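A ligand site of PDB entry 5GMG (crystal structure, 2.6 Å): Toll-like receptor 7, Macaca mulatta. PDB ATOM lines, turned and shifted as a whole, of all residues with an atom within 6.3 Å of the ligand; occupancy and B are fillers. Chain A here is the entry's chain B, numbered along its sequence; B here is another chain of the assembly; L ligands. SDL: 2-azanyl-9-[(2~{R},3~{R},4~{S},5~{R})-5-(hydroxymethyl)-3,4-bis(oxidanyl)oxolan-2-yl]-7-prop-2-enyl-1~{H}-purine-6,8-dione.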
ATOM      1  N   THR A 510     -21.298 -19.907  -7.879  1.00  0.00           N
ATOM      2  CA  THR A 510     -21.017 -18.862  -6.900  1.00  0.00           C
ATOM      3  C   THR A 510     -20.617 -19.451  -5.571  1.00  0.00           C
ATOM      4  O   THR A 510     -21.317 -19.312  -4.593  1.00  0.00           O
ATOM      5  CB  THR A 510     -22.207 -17.882  -6.715  1.00  0.00           C
ATOM      6  OG1 THR A 510     -23.449 -18.604  -6.737  1.00  0.00           O
ATOM      7  CG2 THR A 510     -22.221 -16.882  -7.839  1.00  0.00           C
ATOM      8  N   ASP A 533     -17.128 -17.918 -10.188  1.00  0.00           N
ATOM      9  CA  ASP A 533     -17.855 -16.675 -10.038  1.00  0.00           C
ATOM     10  C   ASP A 533     -17.613 -16.128  -8.639  1.00  0.00           C
ATOM     11  O   ASP A 533     -18.244 -16.571  -7.678  1.00  0.00           O
ATOM     12  CB  ASP A 533     -19.335 -16.928 -10.296  1.00  0.00           C
ATOM     13  CG  ASP A 533     -20.129 -15.674 -10.371  1.00  0.00           C
ATOM     14  OD1 ASP A 533     -19.702 -14.709  -9.699  1.00  0.00           O
ATOM     15  OD2 ASP A 533     -21.156 -15.653 -11.097  1.00  0.00           O
ATOM     16  N   LEU A 534     -16.662 -15.200  -8.530  1.00  0.00           N
ATOM     17  CA  LEU A 534     -16.272 -14.657  -7.235  1.00  0.00           C
ATOM     18  C   LEU A 534     -17.290 -13.586  -6.694  1.00  0.00           C
ATOM     19  O   LEU A 534     -16.940 -12.416  -6.511  1.00  0.00           O
ATOM     20  CB  LEU A 534     -14.822 -14.117  -7.240  1.00  0.00           C
ATOM     21  CG  LEU A 534     -13.680 -14.912  -6.587  1.00  0.00           C
ATOM     22  CD1 LEU A 534     -12.436 -14.043  -6.419  1.00  0.00           C
ATOM     23  CD2 LEU A 534     -14.034 -15.550  -5.248  1.00  0.00           C
ATOM     24  N   LEU A 535     -18.527 -14.020  -6.445  1.00  0.00           N
ATOM     25  CA  LEU A 535     -19.534 -13.133  -5.875  1.00  0.00           C
ATOM     26  C   LEU A 535     -19.346 -12.996  -4.366  1.00  0.00           C
ATOM     27  O   LEU A 535     -19.433 -11.908  -3.845  1.00  0.00           O
ATOM     28  CB  LEU A 535     -20.941 -13.621  -6.185  1.00  0.00           C
ATOM     29  CG  LEU A 535     -22.100 -12.908  -5.500  1.00  0.00           C
ATOM     30  CD1 LEU A 535     -22.090 -11.428  -5.784  1.00  0.00           C
ATOM     31  CD2 LEU A 535     -23.402 -13.547  -5.946  1.00  0.00           C
ATOM     32  N   HIS A 536     -19.072 -14.106  -3.681  1.00  0.00           N
ATOM     33  CA  HIS A 536     -18.961 -14.128  -2.233  1.00  0.00           C
ATOM     34  C   HIS A 536     -17.485 -14.109  -1.841  1.00  0.00           C
ATOM     35  O   HIS A 536     -16.700 -14.898  -2.357  1.00  0.00           O
ATOM     36  CB  HIS A 536     -19.640 -15.395  -1.651  1.00  0.00           C
ATOM     37  CG  HIS A 536     -21.055 -15.612  -2.113  1.00  0.00           C
ATOM     38  ND1 HIS A 536     -22.086 -14.730  -1.857  1.00  0.00           N
ATOM     39  CD2 HIS A 536     -21.616 -16.631  -2.807  1.00  0.00           C
ATOM     40  CE1 HIS A 536     -23.207 -15.182  -2.381  1.00  0.00           C
ATOM     41  NE2 HIS A 536     -22.955 -16.337  -2.964  1.00  0.00           N
ATOM     42  N   GLY A 562     -20.659  -5.290 -15.246  1.00  0.00           N
ATOM     43  CA  GLY A 562     -21.774  -5.288 -14.288  1.00  0.00           C
ATOM     44  C   GLY A 562     -21.760  -6.372 -13.231  1.00  0.00           C
ATOM     45  O   GLY A 562     -22.645  -6.411 -12.369  1.00  0.00           O
ATOM     46  N   ILE A 563     -20.752  -7.242 -13.285  1.00  0.00           N
ATOM     47  CA  ILE A 563     -20.693  -8.468 -12.451  1.00  0.00           C
ATOM     48  C   ILE A 563     -19.808  -8.277 -11.216  1.00  0.00           C
ATOM     49  O   ILE A 563     -18.632  -7.920 -11.304  1.00  0.00           O
ATOM     50  CB  ILE A 563     -20.233  -9.676 -13.276  1.00  0.00           C
ATOM     51  CG1 ILE A 563     -21.154  -9.831 -14.485  1.00  0.00           C
ATOM     52  CG2 ILE A 563     -20.246 -10.935 -12.411  1.00  0.00           C
ATOM     53  CD1 ILE A 563     -21.051 -11.136 -15.255  1.00  0.00           C
ATOM     54  N   THR A 564     -20.380  -8.539 -10.047  1.00  0.00           N
ATOM     55  CA  THR A 564     -19.737  -8.207  -8.779  1.00  0.00           C
ATOM     56  C   THR A 564     -18.710  -9.264  -8.541  1.00  0.00           C
ATOM     57  O   THR A 564     -19.054 -10.443  -8.564  1.00  0.00           O
ATOM     58  CB  THR A 564     -20.786  -8.131  -7.619  1.00  0.00           C
ATOM     59  OG1 THR A 564     -21.717  -7.070  -7.875  1.00  0.00           O
ATOM     60  CG2 THR A 564     -20.151  -7.906  -6.264  1.00  0.00           C
ATOM     61  N   HIS A 565     -17.462  -8.862  -8.346  1.00  0.00           N
ATOM     62  CA  HIS A 565     -16.372  -9.787  -8.021  1.00  0.00           C
ATOM     63  C   HIS A 565     -15.766  -9.328  -6.672  1.00  0.00           C
ATOM     64  O   HIS A 565     -15.734  -8.135  -6.393  1.00  0.00           O
ATOM     65  CB  HIS A 565     -15.284  -9.808  -9.128  1.00  0.00           C
ATOM     66  CG  HIS A 565     -15.806  -9.852 -10.538  1.00  0.00           C
ATOM     67  ND1 HIS A 565     -15.600  -8.832 -11.438  1.00  0.00           N
ATOM     68  CD2 HIS A 565     -16.491 -10.803 -11.218  1.00  0.00           C
ATOM     69  CE1 HIS A 565     -16.152  -9.139 -12.604  1.00  0.00           C
ATOM     70  NE2 HIS A 565     -16.710 -10.327 -12.488  1.00  0.00           N
ATOM     71  N   TYR B 242     -22.547   1.817  -7.844  1.00  0.00           N
ATOM     72  CA  TYR B 242     -22.296   0.407  -7.585  1.00  0.00           C
ATOM     73  C   TYR B 242     -21.529  -0.206  -8.773  1.00  0.00           C
ATOM     74  O   TYR B 242     -22.044  -0.196  -9.910  1.00  0.00           O
ATOM     75  CB  TYR B 242     -23.610  -0.364  -7.362  1.00  0.00           C
ATOM     76  CG  TYR B 242     -23.352  -1.784  -6.853  1.00  0.00           C
ATOM     77  CD1 TYR B 242     -22.752  -1.981  -5.581  1.00  0.00           C
ATOM     78  CD2 TYR B 242     -23.651  -2.915  -7.616  1.00  0.00           C
ATOM     79  CE1 TYR B 242     -22.487  -3.252  -5.091  1.00  0.00           C
ATOM     80  CE2 TYR B 242     -23.398  -4.206  -7.120  1.00  0.00           C
ATOM     81  CZ  TYR B 242     -22.815  -4.368  -5.857  1.00  0.00           C
ATOM     82  OH  TYR B 242     -22.547  -5.611  -5.310  1.00  0.00           O
ATOM     83  N   ASN B 243     -20.331  -0.737  -8.508  1.00  0.00           N
ATOM     84  CA  ASN B 243     -19.412  -1.306  -9.506  1.00  0.00           C
ATOM     85  C   ASN B 243     -19.096  -0.336 -10.642  1.00  0.00           C
ATOM     86  O   ASN B 243     -18.989  -0.732 -11.797  1.00  0.00           O
ATOM     87  CB  ASN B 243     -19.961  -2.630 -10.104  1.00  0.00           C
ATOM     88  CG  ASN B 243     -19.913  -3.799  -9.119  1.00  0.00           C
ATOM     89  OD1 ASN B 243     -19.048  -3.853  -8.218  1.00  0.00           O
ATOM     90  ND2 ASN B 243     -20.831  -4.762  -9.311  1.00  0.00           N
ATOM     91  N   PHE B 329     -31.241  -3.152 -11.120  1.00  0.00           N
ATOM     92  CA  PHE B 329     -31.419  -4.111 -10.038  1.00  0.00           C
ATOM     93  C   PHE B 329     -31.236  -3.485  -8.658  1.00  0.00           C
ATOM     94  O   PHE B 329     -30.578  -2.465  -8.497  1.00  0.00           O
ATOM     95  CB  PHE B 329     -30.536  -5.352 -10.198  1.00  0.00           C
ATOM     96  CG  PHE B 329     -29.056  -5.076 -10.109  1.00  0.00           C
ATOM     97  CD1 PHE B 329     -28.290  -4.861 -11.257  1.00  0.00           C
ATOM     98  CD2 PHE B 329     -28.401  -5.098  -8.888  1.00  0.00           C
ATOM     99  CE1 PHE B 329     -26.916  -4.618 -11.165  1.00  0.00           C
ATOM    100  CE2 PHE B 329     -27.020  -4.861  -8.793  1.00  0.00           C
ATOM    101  CZ  PHE B 329     -26.281  -4.625  -9.933  1.00  0.00           C
ATOM    102  N   GLU B 330     -31.875  -4.105  -7.678  1.00  0.00           N
ATOM    103  CA  GLU B 330     -31.744  -3.724  -6.289  1.00  0.00           C
ATOM    104  C   GLU B 330     -30.533  -4.477  -5.769  1.00  0.00           C
ATOM    105  O   GLU B 330     -30.375  -5.681  -6.063  1.00  0.00           O
ATOM    106  CB  GLU B 330     -33.006  -4.127  -5.505  1.00  0.00           C
ATOM    107  CG  GLU B 330     -34.327  -3.702  -6.157  1.00  0.00           C
ATOM    108  CD  GLU B 330     -35.526  -4.212  -5.395  1.00  0.00           C
ATOM    109  OE1 GLU B 330     -36.231  -5.108  -5.907  1.00  0.00           O
ATOM    110  OE2 GLU B 330     -35.775  -3.727  -4.268  1.00  0.00           O
ATOM    111  N   LEU B 331     -29.671  -3.814  -5.020  1.00  0.00           N
ATOM    112  CA  LEU B 331     -28.435  -4.447  -4.555  1.00  0.00           C
ATOM    113  C   LEU B 331     -28.822  -5.597  -3.635  1.00  0.00           C
ATOM    114  O   LEU B 331     -29.789  -5.463  -2.882  1.00  0.00           O
ATOM    115  CB  LEU B 331     -27.502  -3.482  -3.816  1.00  0.00           C
ATOM    116  CG  LEU B 331     -27.196  -2.085  -4.421  1.00  0.00           C
ATOM    117  CD1 LEU B 331     -25.961  -1.475  -3.784  1.00  0.00           C
ATOM    118  CD2 LEU B 331     -27.051  -2.112  -5.940  1.00  0.00           C
ATOM    119  N   GLN B 332     -28.107  -6.713  -3.724  1.00  0.00           N
ATOM    120  CA  GLN B 332     -28.308  -7.889  -2.843  1.00  0.00           C
ATOM    121  C   GLN B 332     -29.633  -8.642  -3.065  1.00  0.00           C
ATOM    122  O   GLN B 332     -30.029  -9.410  -2.196  1.00  0.00           O
ATOM    123  CB  GLN B 332     -28.216  -7.501  -1.362  1.00  0.00           C
ATOM    124  CG  GLN B 332     -27.054  -6.589  -0.967  1.00  0.00           C
ATOM    125  CD  GLN B 332     -25.682  -7.250  -1.084  1.00  0.00           C
ATOM    126  OE1 GLN B 332     -25.561  -8.439  -1.397  1.00  0.00           O
ATOM    127  NE2 GLN B 332     -24.636  -6.475  -0.813  1.00  0.00           N
ATOM    128  N   VAL B 333     -30.295  -8.466  -4.200  1.00  0.00           N
ATOM    129  CA  VAL B 333     -31.634  -9.041  -4.429  1.00  0.00           C
ATOM    130  C   VAL B 333     -31.749  -9.812  -5.763  1.00  0.00           C
ATOM    131  O   VAL B 333     -31.731  -9.230  -6.868  1.00  0.00           O
ATOM    132  CB  VAL B 333     -32.744  -7.950  -4.361  1.00  0.00           C
ATOM    133  CG1 VAL B 333     -34.116  -8.531  -4.698  1.00  0.00           C
ATOM    134  CG2 VAL B 333     -32.760  -7.260  -2.993  1.00  0.00           C
ATOM    135  N   TYR B 334     -31.953 -11.109  -5.601  1.00  0.00           N
ATOM    136  CA  TYR B 334     -32.202 -12.013  -6.699  1.00  0.00           C
ATOM    137  C   TYR B 334     -33.719 -12.287  -6.808  1.00  0.00           C
ATOM    138  O   TYR B 334     -34.238 -13.254  -6.225  1.00  0.00           O
ATOM    139  CB  TYR B 334     -31.375 -13.297  -6.472  1.00  0.00           C
ATOM    140  CG  TYR B 334     -31.206 -14.261  -7.660  1.00  0.00           C
ATOM    141  CD1 TYR B 334     -31.386 -13.855  -9.011  1.00  0.00           C
ATOM    142  CD2 TYR B 334     -30.851 -15.581  -7.427  1.00  0.00           C
ATOM    143  CE1 TYR B 334     -31.219 -14.749 -10.065  1.00  0.00           C
ATOM    144  CE2 TYR B 334     -30.676 -16.476  -8.466  1.00  0.00           C
ATOM    145  CZ  TYR B 334     -30.853 -16.071  -9.792  1.00  0.00           C
ATOM    146  OH  TYR B 334     -30.639 -16.988 -10.800  1.00  0.00           O
ATOM    147  N   ARG B 335     -34.417 -11.434  -7.550  1.00  0.00           N
ATOM    148  CA  ARG B 335     -35.843 -11.617  -7.848  1.00  0.00           C
ATOM    149  C   ARG B 335     -36.095 -12.956  -8.451  1.00  0.00           C
ATOM    150  O   ARG B 335     -35.284 -13.432  -9.248  1.00  0.00           O
ATOM    151  CB  ARG B 335     -36.381 -10.533  -8.779  1.00  0.00           C
ATOM    152  CG  ARG B 335     -36.557  -9.190  -8.069  1.00  0.00           C
ATOM    153  CD  ARG B 335     -37.219  -8.124  -8.928  1.00  0.00           C
ATOM    154  NE  ARG B 335     -37.434  -6.894  -8.147  1.00  0.00           N
ATOM    155  CZ  ARG B 335     -38.609  -6.282  -7.952  1.00  0.00           C
ATOM    156  NH1 ARG B 335     -39.743  -6.734  -8.482  1.00  0.00           N
ATOM    157  NH2 ARG B 335     -38.639  -5.170  -7.200  1.00  0.00           N
ATOM    158  N   VAL B 359     -31.949  -8.592 -13.009  1.00  0.00           N
ATOM    159  CA  VAL B 359     -31.426  -9.647 -12.108  1.00  0.00           C
ATOM    160  C   VAL B 359     -32.540 -10.532 -11.582  1.00  0.00           C
ATOM    161  O   VAL B 359     -33.069 -10.272 -10.495  1.00  0.00           O
ATOM    162  CB  VAL B 359     -30.532  -9.102 -10.960  1.00  0.00           C
ATOM    163  CG1 VAL B 359     -29.925 -10.236 -10.151  1.00  0.00           C
ATOM    164  CG2 VAL B 359     -29.404  -8.244 -11.513  1.00  0.00           C
ATOM    165  N   PHE B 386     -28.575 -13.035 -14.912  1.00  0.00           N
ATOM    166  CA  PHE B 386     -28.348 -14.223 -14.094  1.00  0.00           C
ATOM    167  C   PHE B 386     -29.520 -15.187 -14.113  1.00  0.00           C
ATOM    168  O   PHE B 386     -29.762 -15.910 -13.154  1.00  0.00           O
ATOM    169  CB  PHE B 386     -27.941 -13.815 -12.699  1.00  0.00           C
ATOM    170  CG  PHE B 386     -26.720 -12.951 -12.689  1.00  0.00           C
ATOM    171  CD1 PHE B 386     -25.457 -13.524 -12.648  1.00  0.00           C
ATOM    172  CD2 PHE B 386     -26.827 -11.560 -12.763  1.00  0.00           C
ATOM    173  CE1 PHE B 386     -24.318 -12.728 -12.667  1.00  0.00           C
ATOM    174  CE2 PHE B 386     -25.691 -10.758 -12.761  1.00  0.00           C
ATOM    175  CZ  PHE B 386     -24.433 -11.345 -12.712  1.00  0.00           C
ATOM    176  N   LYS B 388     -31.390 -18.307 -14.553  1.00  0.00           N
ATOM    177  CA  LYS B 388     -31.078 -19.745 -14.509  1.00  0.00           C
ATOM    178  C   LYS B 388     -32.023 -20.695 -15.288  1.00  0.00           C
ATOM    179  O   LYS B 388     -31.611 -21.793 -15.667  1.00  0.00           O
ATOM    180  CB  LYS B 388     -30.963 -20.220 -13.067  1.00  0.00           C
ATOM    181  CG  LYS B 388     -29.674 -19.760 -12.436  1.00  0.00           C
ATOM    182  CD  LYS B 388     -29.538 -20.200 -10.984  1.00  0.00           C
ATOM    183  CE  LYS B 388     -28.088 -20.189 -10.527  1.00  0.00           C
ATOM    184  NZ  LYS B 388     -27.895 -19.363  -9.311  1.00  0.00           N
ATOM    185  N   LYS B 410     -27.259 -17.518 -16.987  1.00  0.00           N
ATOM    186  CA  LYS B 410     -26.893 -18.723 -16.255  1.00  0.00           C
ATOM    187  C   LYS B 410     -27.865 -19.860 -16.553  1.00  0.00           C
ATOM    188  O   LYS B 410     -27.986 -20.833 -15.801  1.00  0.00           O
ATOM    189  CB  LYS B 410     -26.781 -18.364 -14.753  1.00  0.00           C
ATOM    190  CG  LYS B 410     -25.335 -18.197 -14.276  1.00  0.00           C
ATOM    191  CD  LYS B 410     -25.073 -17.983 -12.797  1.00  0.00           C
ATOM    192  CE  LYS B 410     -23.686 -17.317 -12.611  1.00  0.00           C
ATOM    193  NZ  LYS B 410     -22.626 -18.095 -11.921  1.00  0.00           N
HETATM  194  O5  SDL L   1     -28.351 -12.132  -7.891  1.00  0.00           O
HETATM  195  C5  SDL L   1     -27.166 -12.417  -8.273  1.00  0.00           C
HETATM  196  N1  SDL L   1     -26.831 -13.632  -8.679  1.00  0.00           N
HETATM  197  C10 SDL L   1     -27.675 -14.825  -8.720  1.00  0.00           C
HETATM  198  C11 SDL L   1     -27.366 -15.749  -7.547  1.00  0.00           C
HETATM  199  C12 SDL L   1     -26.808 -15.336  -6.402  1.00  0.00           C
HETATM  200  C6  SDL L   1     -25.530 -13.525  -8.982  1.00  0.00           C
HETATM  201  C9  SDL L   1     -25.092 -12.139  -8.756  1.00  0.00           C
HETATM  202  N4  SDL L   1     -23.799 -11.819  -9.031  1.00  0.00           N
HETATM  203  C8  SDL L   1     -22.924 -12.759  -9.500  1.00  0.00           C
HETATM  204  N3  SDL L   1     -21.655 -12.354  -9.720  1.00  0.00           N
HETATM  205  N2  SDL L   1     -23.288 -14.042  -9.723  1.00  0.00           N
HETATM  206  C7  SDL L   1     -24.539 -14.496  -9.493  1.00  0.00           C
HETATM  207  O4  SDL L   1     -24.846 -15.682  -9.699  1.00  0.00           O
HETATM  208  N   SDL L   1     -26.169 -11.518  -8.287  1.00  0.00           N
HETATM  209  C4  SDL L   1     -26.280 -10.103  -7.947  1.00  0.00           C
HETATM  210  C3  SDL L   1     -25.205  -9.462  -7.056  1.00  0.00           C
HETATM  211  O2  SDL L   1     -25.270  -9.614  -5.629  1.00  0.00           O
HETATM  212  C2  SDL L   1     -25.494  -8.042  -7.503  1.00  0.00           C
HETATM  213  O1  SDL L   1     -26.725  -7.553  -6.910  1.00  0.00           O
HETATM  214  O3  SDL L   1     -26.130  -9.502  -9.232  1.00  0.00           O
HETATM  215  C1  SDL L   1     -25.616  -8.188  -9.034  1.00  0.00           C
HETATM  216  C   SDL L   1     -24.324  -7.970  -9.859  1.00  0.00           C
HETATM  217  O   SDL L   1     -23.286  -8.928  -9.572  1.00  0.00           O
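OH of Tyr 242 of chain B is in hydrogen-bond range of OG1 of Thr 564 (3.1 Å). The side-chain hydroxyl of Thr 564 lies within hydrogen-bond range of the side-chain amide nitrogen of Asn 243 of chain B (2.9 Å). The side-chain amino group (NZ) of Lys 410 of chain B lies within salt-bridge range of the side-chain carboxylate (OD2) of Asp 533, at 3.0 Å. ND1 of His 565 lies close to O of Ile 563 (3.2 Å). OH of Tyr 334 of chain B is in hydrogen-bond range of O of Phe 386 of chain B.
CG2 of Thr 510 touches O4 of the ligand, 3.4 Å away. CD2 of Leu 535 touches N4 of the ligand (3.6 Å). Gly 562 touches the ligand (O to C, 3.4 Å). Ile 563 touches the ligand (CG2 to N3, 3.4 Å). CE2 of Phe 329 of chain B touches O1 of the ligand, at 3.3 Å. Gln 332 of chain B touches the ligand (N to O1, 3.6 Å). Tyr 334 of chain B touches the ligand (CE2 to C10, 3.4 Å). Val 359 of chain B touches the ligand. CE1 of Phe 386 of chain B touches N2 of the ligand, 3.4 Å away. CE of Lys 410 of chain B touches O4 of the ligand, at 3.5 Å. Of the 22 residues printed, 12 come within 4 Å of the ligand. The nearest printed residue that does not touch the ligand is Lys 388 of chain B (4.1 Å).
An oxygen (O) of the ligand is in hydrogen-bond range of the backbone NH (N) of Thr 564 (3.0 Å). N3 of the ligand sits at hydrogen-bond distance from O of Thr 564, 3.4 Å away. O of the ligand sits at hydrogen-bond distance from OG1 of Thr 564, 3.0 Å away. A nitrogen (N2) of the ligand is in hydrogen-bond range of the side-chain carboxylate (OD2) of Asp 533, at 3.0 Å.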
